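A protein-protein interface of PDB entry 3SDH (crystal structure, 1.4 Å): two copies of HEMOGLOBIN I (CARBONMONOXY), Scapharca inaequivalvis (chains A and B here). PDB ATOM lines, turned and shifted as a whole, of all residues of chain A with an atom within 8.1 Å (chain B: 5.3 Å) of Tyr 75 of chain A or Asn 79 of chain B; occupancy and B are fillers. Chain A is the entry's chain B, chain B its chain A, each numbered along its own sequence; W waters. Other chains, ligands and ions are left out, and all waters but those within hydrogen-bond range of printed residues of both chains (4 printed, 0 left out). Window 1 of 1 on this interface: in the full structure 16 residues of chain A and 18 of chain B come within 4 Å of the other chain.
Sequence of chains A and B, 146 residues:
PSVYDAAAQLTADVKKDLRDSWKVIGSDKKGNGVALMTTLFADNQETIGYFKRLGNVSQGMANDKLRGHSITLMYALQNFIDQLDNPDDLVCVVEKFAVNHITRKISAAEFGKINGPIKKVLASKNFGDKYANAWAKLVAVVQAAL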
ATOM      1  N   TRP A  22      11.280  29.884  -6.601  1.00  0.00           N
ATOM      2  CA  TRP A  22      10.321  28.869  -6.158  1.00  0.00           C
ATOM      3  C   TRP A  22       9.439  29.376  -5.019  1.00  0.00           C
ATOM      4  O   TRP A  22       8.240  29.028  -4.922  1.00  0.00           O
ATOM      5  CB  TRP A  22      11.003  27.567  -5.741  1.00  0.00           C
ATOM      6  CG  TRP A  22       9.979  26.501  -5.428  1.00  0.00           C
ATOM      7  CD1 TRP A  22       9.724  25.975  -4.194  1.00  0.00           C
ATOM      8  CD2 TRP A  22       9.091  25.861  -6.344  1.00  0.00           C
ATOM      9  NE1 TRP A  22       8.722  25.030  -4.300  1.00  0.00           N
ATOM     10  CE2 TRP A  22       8.336  24.912  -5.603  1.00  0.00           C
ATOM     11  CE3 TRP A  22       8.886  26.014  -7.718  1.00  0.00           C
ATOM     12  CZ2 TRP A  22       7.334  24.177  -6.221  1.00  0.00           C
ATOM     13  CZ3 TRP A  22       7.880  25.247  -8.321  1.00  0.00           C
ATOM     14  CH2 TRP A  22       7.158  24.304  -7.578  1.00  0.00           C
ATOM     15  N   GLY A  26       6.119  28.508  -6.488  1.00  0.00           N
ATOM     16  CA  GLY A  26       5.632  27.318  -5.765  1.00  0.00           C
ATOM     17  C   GLY A  26       4.539  27.674  -4.743  1.00  0.00           C
ATOM     18  O   GLY A  26       4.034  26.745  -4.056  1.00  0.00           O
ATOM     19  N   LYS A  29       0.462  26.413  -6.259  1.00  0.00           N
ATOM     20  CA  LYS A  29       0.759  25.222  -7.075  1.00  0.00           C
ATOM     21  C   LYS A  29      -0.343  24.916  -8.058  1.00  0.00           C
ATOM     22  O   LYS A  29      -0.022  24.529  -9.222  1.00  0.00           O
ATOM     23  CB  LYS A  29       1.035  24.026  -6.136  1.00  0.00           C
ATOM     24  CG  LYS A  29       2.402  24.228  -5.415  1.00  0.00           C
ATOM     25  CD  LYS A  29       2.681  22.988  -4.564  1.00  0.00           C
ATOM     26  CE  LYS A  29       4.089  23.021  -3.971  1.00  0.00           C
ATOM     27  NZ  LYS A  29       4.234  24.125  -3.002  1.00  0.00           N
ATOM     28  N   LYS A  30      -1.609  25.030  -7.665  1.00  0.00           N
ATOM     29  CA  LYS A  30      -2.712  24.793  -8.595  1.00  0.00           C
ATOM     30  C   LYS A  30      -2.665  25.777  -9.780  1.00  0.00           C
ATOM     31  O   LYS A  30      -2.683  25.373 -10.978  1.00  0.00           O
ATOM     32  CB  LYS A  30      -4.047  24.970  -7.853  1.00  0.00           C
ATOM     33  CG  LYS A  30      -5.238  24.830  -8.787  1.00  0.00           C
ATOM     34  CD  LYS A  30      -6.554  24.676  -8.021  1.00  0.00           C
ATOM     35  CE  LYS A  30      -6.897  25.783  -7.092  1.00  0.00           C
ATOM     36  NZ  LYS A  30      -8.294  25.568  -6.524  1.00  0.00           N
ATOM     37  N   GLY A  33       0.823  25.470 -11.680  1.00  0.00           N
ATOM     38  CA  GLY A  33       0.969  24.132 -12.322  1.00  0.00           C
ATOM     39  C   GLY A  33       0.077  24.085 -13.559  1.00  0.00           C
ATOM     40  O   GLY A  33       0.530  23.601 -14.629  1.00  0.00           O
ATOM     41  N   ARG A  67      -6.112  19.066 -13.459  1.00  0.00           N
ATOM     42  CA  ARG A  67      -5.809  19.854 -12.227  1.00  0.00           C
ATOM     43  C   ARG A  67      -5.056  18.915 -11.277  1.00  0.00           C
ATOM     44  O   ARG A  67      -4.024  19.372 -10.769  1.00  0.00           O
ATOM     45  CB  ARG A  67      -7.116  20.362 -11.626  1.00  0.00           C
ATOM     46  CG  ARG A  67      -6.901  21.450 -10.581  1.00  0.00           C
ATOM     47  CD  ARG A  67      -8.243  22.129 -10.332  1.00  0.00           C
ATOM     48  NE  ARG A  67      -9.044  21.236  -9.471  1.00  0.00           N
ATOM     49  CZ  ARG A  67     -10.164  20.662  -9.949  1.00  0.00           C
ATOM     50  NH1 ARG A  67     -10.651  20.859 -11.185  1.00  0.00           N
ATOM     51  NH2 ARG A  67     -10.861  19.781  -9.185  1.00  0.00           N
ATOM     52  N   GLY A  68      -5.451  17.658 -11.104  1.00  0.00           N
ATOM     53  CA  GLY A  68      -4.762  16.749 -10.182  1.00  0.00           C
ATOM     54  C   GLY A  68      -3.317  16.461 -10.614  1.00  0.00           C
ATOM     55  O   GLY A  68      -2.331  16.418  -9.854  1.00  0.00           O
ATOM     56  N   HIS A  69      -3.175  16.267 -11.948  1.00  0.00           N
ATOM     57  CA  HIS A  69      -1.817  16.063 -12.514  1.00  0.00           C
ATOM     58  C   HIS A  69      -0.954  17.302 -12.271  1.00  0.00           C
ATOM     59  O   HIS A  69       0.251  17.181 -11.952  1.00  0.00           O
ATOM     60  CB  HIS A  69      -1.951  15.799 -14.069  1.00  0.00           C
ATOM     61  CG  HIS A  69      -0.635  15.921 -14.768  1.00  0.00           C
ATOM     62  ND1 HIS A  69       0.266  14.887 -14.848  1.00  0.00           N
ATOM     63  CD2 HIS A  69      -0.115  16.998 -15.399  1.00  0.00           C
ATOM     64  CE1 HIS A  69       1.353  15.357 -15.512  1.00  0.00           C
ATOM     65  NE2 HIS A  69       1.135  16.637 -15.851  1.00  0.00           N
ATOM     66  N   SER A  70      -1.496  18.491 -12.567  1.00  0.00           N
ATOM     67  CA  SER A  70      -0.708  19.734 -12.495  1.00  0.00           C
ATOM     68  C   SER A  70      -0.248  20.095 -11.059  1.00  0.00           C
ATOM     69  O   SER A  70       0.876  20.544 -10.866  1.00  0.00           O
ATOM     70  CB  SER A  70      -1.547  20.881 -13.029  1.00  0.00           C
ATOM     71  OG  SER A  70      -1.838  20.604 -14.405  1.00  0.00           O
ATOM     72  N   ILE A  71      -1.168  19.891 -10.112  1.00  0.00           N
ATOM     73  CA  ILE A  71      -0.774  20.097  -8.688  1.00  0.00           C
ATOM     74  C   ILE A  71       0.371  19.137  -8.339  1.00  0.00           C
ATOM     75  O   ILE A  71       1.382  19.483  -7.695  1.00  0.00           O
ATOM     76  CB  ILE A  71      -2.009  19.872  -7.749  1.00  0.00           C
ATOM     77  CG1 ILE A  71      -3.044  20.989  -7.949  1.00  0.00           C
ATOM     78  CG2 ILE A  71      -1.501  19.773  -6.266  1.00  0.00           C
ATOM     79  CD1 ILE A  71      -4.447  20.718  -7.320  1.00  0.00           C
ATOM     80  N   THR A  72       0.169  17.855  -8.753  1.00  0.00           N
ATOM     81  CA  THR A  72       1.169  16.845  -8.414  1.00  0.00           C
ATOM     82  C   THR A  72       2.535  17.138  -9.022  1.00  0.00           C
ATOM     83  O   THR A  72       3.623  16.949  -8.459  1.00  0.00           O
ATOM     84  CB  THR A  72       0.682  15.379  -8.774  1.00  0.00           C
ATOM     85  OG1 THR A  72      -0.545  15.228  -8.016  1.00  0.00           O
ATOM     86  CG2 THR A  72       1.714  14.301  -8.467  1.00  0.00           C
ATOM     87  N   LEU A  73       2.465  17.645 -10.302  1.00  0.00           N
ATOM     88  CA  LEU A  73       3.775  17.994 -10.933  1.00  0.00           C
ATOM     89  C   LEU A  73       4.513  19.032 -10.070  1.00  0.00           C
ATOM     90  O   LEU A  73       5.754  18.996  -9.940  1.00  0.00           O
ATOM     91  CB  LEU A  73       3.506  18.457 -12.404  1.00  0.00           C
ATOM     92  CG  LEU A  73       4.751  18.919 -13.162  1.00  0.00           C
ATOM     93  CD1 LEU A  73       4.528  18.653 -14.666  1.00  0.00           C
ATOM     94  CD2 LEU A  73       4.932  20.408 -12.928  1.00  0.00           C
ATOM     95  N   MET A  74       3.766  19.999  -9.525  1.00  0.00           N
ATOM     96  CA  MET A  74       4.387  21.054  -8.691  1.00  0.00           C
ATOM     97  C   MET A  74       5.016  20.473  -7.413  1.00  0.00           C
ATOM     98  O   MET A  74       6.036  21.025  -6.948  1.00  0.00           O
ATOM     99  CB  MET A  74       3.423  22.174  -8.375  1.00  0.00           C
ATOM    100  CG  MET A  74       2.901  22.900  -9.608  1.00  0.00           C
ATOM    101  SD  MET A  74       4.262  23.801 -10.474  1.00  0.00           S
ATOM    102  CE  MET A  74       4.252  25.332  -9.503  1.00  0.00           C
ATOM    103  N   TYR A  75       4.502  19.352  -6.923  1.00  0.00           N
ATOM    104  CA  TYR A  75       5.159  18.700  -5.768  1.00  0.00           C
ATOM    105  C   TYR A  75       6.411  17.940  -6.198  1.00  0.00           C
ATOM    106  O   TYR A  75       7.314  17.680  -5.347  1.00  0.00           O
ATOM    107  CB  TYR A  75       4.166  17.767  -5.037  1.00  0.00           C
ATOM    108  CG  TYR A  75       3.277  18.636  -4.176  1.00  0.00           C
ATOM    109  CD1 TYR A  75       3.664  19.037  -2.894  1.00  0.00           C
ATOM    110  CD2 TYR A  75       2.028  19.029  -4.634  1.00  0.00           C
ATOM    111  CE1 TYR A  75       2.845  19.893  -2.126  1.00  0.00           C
ATOM    112  CE2 TYR A  75       1.204  19.873  -3.920  1.00  0.00           C
ATOM    113  CZ  TYR A  75       1.578  20.256  -2.622  1.00  0.00           C
ATOM    114  OH  TYR A  75       0.808  21.090  -1.895  1.00  0.00           O
ATOM    115  N   ALA A  76       6.492  17.521  -7.476  1.00  0.00           N
ATOM    116  CA  ALA A  76       7.783  16.914  -7.921  1.00  0.00           C
ATOM    117  C   ALA A  76       8.817  18.010  -7.894  1.00  0.00           C
ATOM    118  O   ALA A  76       9.984  17.806  -7.514  1.00  0.00           O
ATOM    119  CB  ALA A  76       7.700  16.264  -9.310  1.00  0.00           C
ATOM    120  N   LEU A  77       8.452  19.225  -8.376  1.00  0.00           N
ATOM    121  CA  LEU A  77       9.425  20.329  -8.303  1.00  0.00           C
ATOM    122  C   LEU A  77       9.734  20.726  -6.830  1.00  0.00           C
ATOM    123  O   LEU A  77      10.920  21.027  -6.576  1.00  0.00           O
ATOM    124  CB  LEU A  77       8.909  21.517  -9.128  1.00  0.00           C
ATOM    125  CG  LEU A  77       8.678  21.226 -10.631  1.00  0.00           C
ATOM    126  CD1 LEU A  77       8.155  22.484 -11.333  1.00  0.00           C
ATOM    127  CD2 LEU A  77      10.017  20.828 -11.234  1.00  0.00           C
ATOM    128  N   GLN A  78       8.723  20.702  -5.996  1.00  0.00           N
ATOM    129  CA  GLN A  78       8.982  20.963  -4.543  1.00  0.00           C
ATOM    130  C   GLN A  78      10.042  20.011  -4.007  1.00  0.00           C
ATOM    131  O   GLN A  78      11.015  20.409  -3.355  1.00  0.00           O
ATOM    132  CB  GLN A  78       7.665  20.820  -3.779  1.00  0.00           C
ATOM    133  CG  GLN A  78       7.836  21.145  -2.298  1.00  0.00           C
ATOM    134  CD  GLN A  78       8.094  22.597  -2.044  1.00  0.00           C
ATOM    135  OE1 GLN A  78       7.283  23.446  -2.475  1.00  0.00           O
ATOM    136  NE2 GLN A  78       9.228  22.889  -1.377  1.00  0.00           N
ATOM    137  N   ASN A  79       9.887  18.764  -4.410  1.00  0.00           N
ATOM    138  CA  ASN A  79      10.777  17.689  -3.957  1.00  0.00           C
ATOM    139  C   ASN A  79      12.221  18.006  -4.366  1.00  0.00           C
ATOM    140  O   ASN A  79      13.193  18.068  -3.624  1.00  0.00           O
ATOM    141  CB  ASN A  79      10.257  16.404  -4.498  1.00  0.00           C
ATOM    142  CG  ASN A  79      10.938  15.126  -4.031  1.00  0.00           C
ATOM    143  OD1 ASN A  79      12.037  15.188  -3.458  1.00  0.00           O
ATOM    144  ND2 ASN A  79      10.278  14.020  -4.419  1.00  0.00           N
ATOM    145  N   PHE A  80      12.348  18.356  -5.690  1.00  0.00           N
ATOM    146  CA  PHE A  80      13.704  18.682  -6.201  1.00  0.00           C
ATOM    147  C   PHE A  80      14.278  19.872  -5.426  1.00  0.00           C
ATOM    148  O   PHE A  80      15.475  19.809  -5.047  1.00  0.00           O
ATOM    149  CB  PHE A  80      13.615  19.082  -7.698  1.00  0.00           C
ATOM    150  CG  PHE A  80      13.227  17.988  -8.660  1.00  0.00           C
ATOM    151  CD1 PHE A  80      13.217  16.646  -8.308  1.00  0.00           C
ATOM    152  CD2 PHE A  80      12.898  18.373  -9.963  1.00  0.00           C
ATOM    153  CE1 PHE A  80      12.824  15.653  -9.226  1.00  0.00           C
ATOM    154  CE2 PHE A  80      12.541  17.407 -10.910  1.00  0.00           C
ATOM    155  CZ  PHE A  80      12.507  16.053 -10.523  1.00  0.00           C
ATOM    156  N   ILE A  81      13.532  20.923  -5.270  1.00  0.00           N
ATOM    157  CA  ILE A  81      13.984  22.138  -4.574  1.00  0.00           C
ATOM    158  C   ILE A  81      14.445  21.791  -3.138  1.00  0.00           C
ATOM    159  O   ILE A  81      15.555  22.220  -2.749  1.00  0.00           O
ATOM    160  CB  ILE A  81      12.912  23.257  -4.592  1.00  0.00           C
ATOM    161  CG1 ILE A  81      12.640  23.733  -6.036  1.00  0.00           C
ATOM    162  CG2 ILE A  81      13.381  24.475  -3.699  1.00  0.00           C
ATOM    163  CD1 ILE A  81      13.946  24.296  -6.685  1.00  0.00           C
ATOM    164  N   ASP A  82      13.654  20.955  -2.456  1.00  0.00           N
ATOM    165  CA  ASP A  82      14.029  20.560  -1.074  1.00  0.00           C
ATOM    166  C   ASP A  82      15.321  19.737  -1.051  1.00  0.00           C
ATOM    167  O   ASP A  82      15.962  19.771   0.034  1.00  0.00           O
ATOM    168  CB  ASP A  82      12.876  19.838  -0.390  1.00  0.00           C
ATOM    169  CG  ASP A  82      11.697  20.727  -0.111  1.00  0.00           C
ATOM    170  OD1 ASP A  82      11.778  21.970  -0.146  1.00  0.00           O
ATOM    171  OD2 ASP A  82      10.620  20.157   0.156  1.00  0.00           O
ATOM    172  N   GLN A  83      15.677  19.008  -2.083  1.00  0.00           N
ATOM    173  CA  GLN A  83      16.860  18.156  -2.092  1.00  0.00           C
ATOM    174  C   GLN A  83      18.158  18.831  -2.606  1.00  0.00           C
ATOM    175  O   GLN A  83      19.202  18.133  -2.675  1.00  0.00           O
ATOM    176  CB  GLN A  83      16.703  16.875  -2.941  1.00  0.00           C
ATOM    177  CG  GLN A  83      15.454  16.062  -2.751  1.00  0.00           C
ATOM    178  CD  GLN A  83      15.005  15.962  -1.314  1.00  0.00           C
ATOM    179  OE1 GLN A  83      15.794  15.796  -0.383  1.00  0.00           O
ATOM    180  NE2 GLN A  83      13.679  16.122  -1.105  1.00  0.00           N
ATOM    181  N   PHE A  97      11.695  10.048 -10.905  1.00  0.00           N
ATOM    182  CA  PHE A  97      10.820  10.709 -11.901  1.00  0.00           C
ATOM    183  C   PHE A  97      11.239  10.397 -13.334  1.00  0.00           C
ATOM    184  O   PHE A  97      10.411  10.398 -14.265  1.00  0.00           O
ATOM    185  CB  PHE A  97      10.675  12.233 -11.647  1.00  0.00           C
ATOM    186  CG  PHE A  97       9.825  12.498 -10.400  1.00  0.00           C
ATOM    187  CD1 PHE A  97       8.469  12.230 -10.418  1.00  0.00           C
ATOM    188  CD2 PHE A  97      10.432  13.017  -9.252  1.00  0.00           C
ATOM    189  CE1 PHE A  97       7.681  12.431  -9.269  1.00  0.00           C
ATOM    190  CE2 PHE A  97       9.667  13.211  -8.086  1.00  0.00           C
ATOM    191  CZ  PHE A  97       8.303  12.937  -8.114  1.00  0.00           C
ATOM    192  N   MET B  74       6.392  10.641   0.622  1.00  0.00           N
ATOM    193  CA  MET B  74       6.092  11.667   1.681  1.00  0.00           C
ATOM    194  C   MET B  74       5.576  12.967   1.048  1.00  0.00           C
ATOM    195  O   MET B  74       4.754  13.646   1.700  1.00  0.00           O
ATOM    196  CB  MET B  74       7.275  11.919   2.597  1.00  0.00           C
ATOM    197  CG  MET B  74       7.699  10.657   3.345  1.00  0.00           C
ATOM    198  SD  MET B  74       6.419  10.170   4.572  1.00  0.00           S
ATOM    199  CE  MET B  74       6.874  11.290   5.910  1.00  0.00           C
ATOM    200  N   TYR B  75       6.039  13.275  -0.172  1.00  0.00           N
ATOM    201  CA  TYR B  75       5.408  14.422  -0.879  1.00  0.00           C
ATOM    202  C   TYR B  75       3.978  14.173  -1.348  1.00  0.00           C
ATOM    203  O   TYR B  75       3.229  15.164  -1.531  1.00  0.00           O
ATOM    204  CB  TYR B  75       6.272  14.908  -2.064  1.00  0.00           C
ATOM    205  CG  TYR B  75       7.500  15.613  -1.542  1.00  0.00           C
ATOM    206  CD1 TYR B  75       7.401  16.967  -1.201  1.00  0.00           C
ATOM    207  CD2 TYR B  75       8.697  14.967  -1.294  1.00  0.00           C
ATOM    208  CE1 TYR B  75       8.491  17.669  -0.656  1.00  0.00           C
ATOM    209  CE2 TYR B  75       9.789  15.643  -0.740  1.00  0.00           C
ATOM    210  CZ  TYR B  75       9.698  17.011  -0.431  1.00  0.00           C
ATOM    211  OH  TYR B  75      10.784  17.653   0.104  1.00  0.00           O
ATOM    212  N   ALA B  76       3.596  12.904  -1.577  1.00  0.00           N
ATOM    213  CA  ALA B  76       2.150  12.664  -1.813  1.00  0.00           C
ATOM    214  C   ALA B  76       1.333  13.024  -0.547  1.00  0.00           C
ATOM    215  O   ALA B  76       0.268  13.644  -0.616  1.00  0.00           O
ATOM    216  CB  ALA B  76       1.927  11.199  -2.251  1.00  0.00           C
ATOM    217  N   LEU B  77       1.861  12.560   0.612  1.00  0.00           N
ATOM    218  CA  LEU B  77       1.176  12.958   1.862  1.00  0.00           C
ATOM    219  C   LEU B  77       1.135  14.495   2.034  1.00  0.00           C
ATOM    220  O   LEU B  77       0.103  15.018   2.449  1.00  0.00           O
ATOM    221  CB  LEU B  77       1.802  12.234   3.068  1.00  0.00           C
ATOM    222  CG  LEU B  77       1.709  10.698   2.984  1.00  0.00           C
ATOM    223  CD1 LEU B  77       2.309  10.107   4.257  1.00  0.00           C
ATOM    224  CD2 LEU B  77       0.264  10.285   2.821  1.00  0.00           C
ATOM    225  N   GLN B  78       2.260  15.131   1.772  1.00  0.00           N
ATOM    226  CA  GLN B  78       2.307  16.635   1.871  1.00  0.00           C
ATOM    227  C   GLN B  78       1.200  17.285   1.034  1.00  0.00           C
ATOM    228  O   GLN B  78       0.505  18.234   1.404  1.00  0.00           O
ATOM    229  CB  GLN B  78       3.703  17.091   1.515  1.00  0.00           C
ATOM    230  CG  GLN B  78       3.787  18.627   1.476  1.00  0.00           C
ATOM    231  CD  GLN B  78       3.842  19.148   2.875  1.00  0.00           C
ATOM    232  OE1 GLN B  78       4.741  18.749   3.634  1.00  0.00           O
ATOM    233  NE2 GLN B  78       2.862  20.002   3.226  1.00  0.00           N
ATOM    234  N   ASN B  79       1.087  16.765  -0.202  1.00  0.00           N
ATOM    235  CA  ASN B  79       0.077  17.194  -1.168  1.00  0.00           C
ATOM    236  C   ASN B  79      -1.349  17.090  -0.562  1.00  0.00           C
ATOM    237  O   ASN B  79      -2.096  18.062  -0.495  1.00  0.00           O
ATOM    238  CB  ASN B  79       0.322  16.378  -2.446  1.00  0.00           C
ATOM    239  CG  ASN B  79      -0.532  16.805  -3.630  1.00  0.00           C
ATOM    240  OD1 ASN B  79      -1.497  17.575  -3.510  1.00  0.00           O
ATOM    241  ND2 ASN B  79      -0.184  16.205  -4.804  1.00  0.00           N
ATOM    242  N   PHE B  80      -1.633  15.871  -0.018  1.00  0.00           N
ATOM    243  CA  PHE B  80      -2.965  15.704   0.601  1.00  0.00           C
ATOM    244  C   PHE B  80      -3.230  16.754   1.723  1.00  0.00           C
ATOM    245  O   PHE B  80      -4.337  17.310   1.762  1.00  0.00           O
ATOM    246  CB  PHE B  80      -3.119  14.307   1.188  1.00  0.00           C
ATOM    247  CG  PHE B  80      -3.054  13.153   0.206  1.00  0.00           C
ATOM    248  CD1 PHE B  80      -3.298  13.347  -1.148  1.00  0.00           C
ATOM    249  CD2 PHE B  80      -2.806  11.865   0.698  1.00  0.00           C
ATOM    250  CE1 PHE B  80      -3.262  12.261  -2.036  1.00  0.00           C
ATOM    251  CE2 PHE B  80      -2.740  10.779  -0.182  1.00  0.00           C
ATOM    252  CZ  PHE B  80      -2.990  10.968  -1.539  1.00  0.00           C
ATOM    253  N   ILE B  81      -2.227  16.888   2.593  1.00  0.00           N
ATOM    254  CA  ILE B  81      -2.437  17.819   3.741  1.00  0.00           C
ATOM    255  C   ILE B  81      -2.669  19.231   3.206  1.00  0.00           C
ATOM    256  O   ILE B  81      -3.530  19.935   3.719  1.00  0.00           O
ATOM    257  CB  ILE B  81      -1.132  17.792   4.638  1.00  0.00           C
ATOM    258  CG1 ILE B  81      -0.948  16.395   5.280  1.00  0.00           C
ATOM    259  CG2 ILE B  81      -1.162  18.910   5.720  1.00  0.00           C
ATOM    260  CD1 ILE B  81      -2.087  15.926   6.189  1.00  0.00           C
ATOM    261  N   ASP B  82      -1.889  19.598   2.163  1.00  0.00           N
ATOM    262  CA  ASP B  82      -2.060  20.991   1.627  1.00  0.00           C
ATOM    263  C   ASP B  82      -3.444  21.157   0.976  1.00  0.00           C
ATOM    264  O   ASP B  82      -3.869  22.346   0.851  1.00  0.00           O
ATOM    265  CB  ASP B  82      -0.946  21.302   0.621  1.00  0.00           C
ATOM    266  CG  ASP B  82       0.401  21.572   1.237  1.00  0.00           C
ATOM    267  OD1 ASP B  82       0.442  21.843   2.465  1.00  0.00           O
ATOM    268  OD2 ASP B  82       1.435  21.541   0.538  1.00  0.00           O
ATOM    269  N   GLN B  83      -4.073  20.088   0.539  1.00  0.00           N
ATOM    270  CA  GLN B  83      -5.398  20.183  -0.080  1.00  0.00           C
ATOM    271  C   GLN B  83      -6.571  20.054   0.897  1.00  0.00           C
ATOM    272  O   GLN B  83      -7.709  20.065   0.373  1.00  0.00           O
ATOM    273  CB  GLN B  83      -5.662  19.142  -1.190  1.00  0.00           C
ATOM    274  CG  GLN B  83      -4.564  19.006  -2.201  1.00  0.00           C
ATOM    275  CD  GLN B  83      -3.970  20.309  -2.655  1.00  0.00           C
ATOM    276  OE1 GLN B  83      -4.695  21.271  -2.851  1.00  0.00           O
ATOM    277  NE2 GLN B  83      -2.632  20.401  -2.666  1.00  0.00           N
ATOM    278  N   VAL B  93      -6.523  15.094  -6.510  1.00  0.00           N
ATOM    279  CA  VAL B  93      -5.127  14.577  -6.294  1.00  0.00           C
ATOM    280  C   VAL B  93      -5.223  13.128  -5.807  1.00  0.00           C
ATOM    281  O   VAL B  93      -4.409  12.287  -6.190  1.00  0.00           O
ATOM    282  CB  VAL B  93      -4.270  15.454  -5.398  1.00  0.00           C
ATOM    283  CG1 VAL B  93      -4.111  16.867  -5.998  1.00  0.00           C
ATOM    284  CG2 VAL B  93      -4.750  15.495  -3.981  1.00  0.00           C
ATOM    285  N   PHE B  97      -3.439   9.694  -7.585  1.00  0.00           N
ATOM    286  CA  PHE B  97      -2.626   8.644  -6.939  1.00  0.00           C
ATOM    287  C   PHE B  97      -3.333   7.294  -6.958  1.00  0.00           C
ATOM    288  O   PHE B  97      -2.660   6.239  -7.012  1.00  0.00           O
ATOM    289  CB  PHE B  97      -2.164   9.018  -5.506  1.00  0.00           C
ATOM    290  CG  PHE B  97      -1.139  10.133  -5.545  1.00  0.00           C
ATOM    291  CD1 PHE B  97       0.110   9.896  -6.107  1.00  0.00           C
ATOM    292  CD2 PHE B  97      -1.462  11.400  -5.069  1.00  0.00           C
ATOM    293  CE1 PHE B  97       1.094  10.917  -6.166  1.00  0.00           C
ATOM    294  CE2 PHE B  97      -0.503  12.419  -5.101  1.00  0.00           C
ATOM    295  CZ  PHE B  97       0.757  12.196  -5.658  1.00  0.00           C
HETATM  296  O   HOH W   1      10.396  18.838   3.108  1.00  0.00           O
HETATM  297  O   HOH W   2      12.618  16.681   2.026  1.00  0.00           O
HETATM  298  O   HOH W   3      -0.934  23.262  -2.684  1.00  0.00           O
HETATM  299  O   HOH W   4       1.730  24.223  -0.915  1.00  0.00           O
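The side-chain hydroxyl (OH) of Tyr 75 of chain B lies within hydrogen-bond range of the side-chain carboxylate (OD2) of Asp 82 of chain A (2.5 Å).
The side-chain hydroxyl (OH) of Tyr 75 of chain B sits at hydrogen-bond distance from the side-chain amide nitrogen (NE2) of Gln 83 of chain A, 3.5 Å away.
The side-chain hydroxyl of Tyr 75 of chain A lies within hydrogen-bond range of the side-chain carboxylate of Asp 82 of chain B, 2.6 Å away.
The side-chain amide nitrogen (ND2) of Asn 79 of chain B sits at hydrogen-bond distance from the side-chain hydroxyl (OG1) of Thr 72 of chain A, at 3.4 Å.
NE2 of Gln 78 of chain A is in hydrogen-bond range of OD1 of Asp 82 of chain A (3.0 Å).
The side-chain amide nitrogen (NE2) of Gln 83 of chain A lies within hydrogen-bond range of the side-chain amide oxygen (OD1) of Asn 79 of chain A (3.0 Å).
NZ of Lys 29 of chain A sits at hydrogen-bond distance from OE1 of Gln 78 of chain A.
OD1 of Asn 79 of chain B sits at hydrogen-bond distance from NE2 of Gln 83 of chain B (3.2 Å).
Among the printed residues, merely in contact across the chains: Asn 79 of chain A with Tyr 75 of chain B (3.5 Å), Ile 71 of chain A with Asn 79 of chain B (3.5 Å), Tyr 75 of chain A with Asn 79 of chain B (3.5 Å), Tyr 75 of chain A with Gln 83 of chain B (3.6 Å), Thr 72 of chain A with Phe 97 of chain B (3.6 Å), Ile 71 of chain A with Gln 83 of chain B (3.8 Å), Gln 78 of chain A with Tyr 75 of chain B (3.9 Å), Ile 71 of chain A with Val 93 of chain B (3.9 Å) and Tyr 75 of chain A with Gln 78 of chain B (3.9 Å).
Asn 79 of chain B touches just these residues of chain A: Ile 71 (3.5 Å), Thr 72 (3.4 Å) and Tyr 75 (3.5 Å).
Of the printed residues of chain A, Phe 97 of chain B touches Thr 72 (3.6 Å).
Printed residues of chain A within 4 Å of Tyr 75 of chain B: Gln 78, Asn 79, Asp 82 and Gln 83.
Printed residues of chain A within 4 Å of Val 93 of chain B: Ile 71.
Leu 73 of chain A touches none of the printed residues of chain B.
Leu 77 of chain A touches none of the printed residues of chain B.
The nearest residue of chain B that does not touch Tyr 75 of chain A is Tyr 75 of chain B (4.1 Å).
The nearest printed residue of chain A that does not touch Asp 82 of chain B is Lys 29 of chain A (5.2 Å).
Of the 23 printed residues of chain A, 7 touch a printed residue of chain B.
Hydrophobic or aromatic side chains of chain A that line the printed part of chain B: Ile 71 and Tyr 75.
Of the 12 printed residues of chain B, 7 touch a printed residue of chain A.
Among the printed residues, no Asp or Glu carboxylate lies within 4 Å of a Lys or Arg side-chain nitrogen of the other chain.
Tyr 75 of chain A touches Gln 78 of chain B, and with the chains exchanged Gln 78 of chain A touches Tyr 75 of chain B.
Tyr 75 of chain A touches Asp 82 of chain B, and with the chains exchanged Asp 82 of chain A touches Tyr 75 of chain B.
11 positions are printed for both chains.
Of the 13 pairs that touch across the chains among the printed residues, 8 have their exchanged pair printed and touching as well.
Water W2 lies within hydrogen-bond range of OH of Tyr 75 of chain B (2.8 Å) and NE2 of Gln 83 of chain A (3.4 Å).
Water W1 lies within hydrogen-bond range of the side-chain carboxylate (OD2) of Asp 82 of chain A (3.2 Å) and the side-chain hydroxyl (OH) of Tyr 75 of chain B (3.3 Å).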
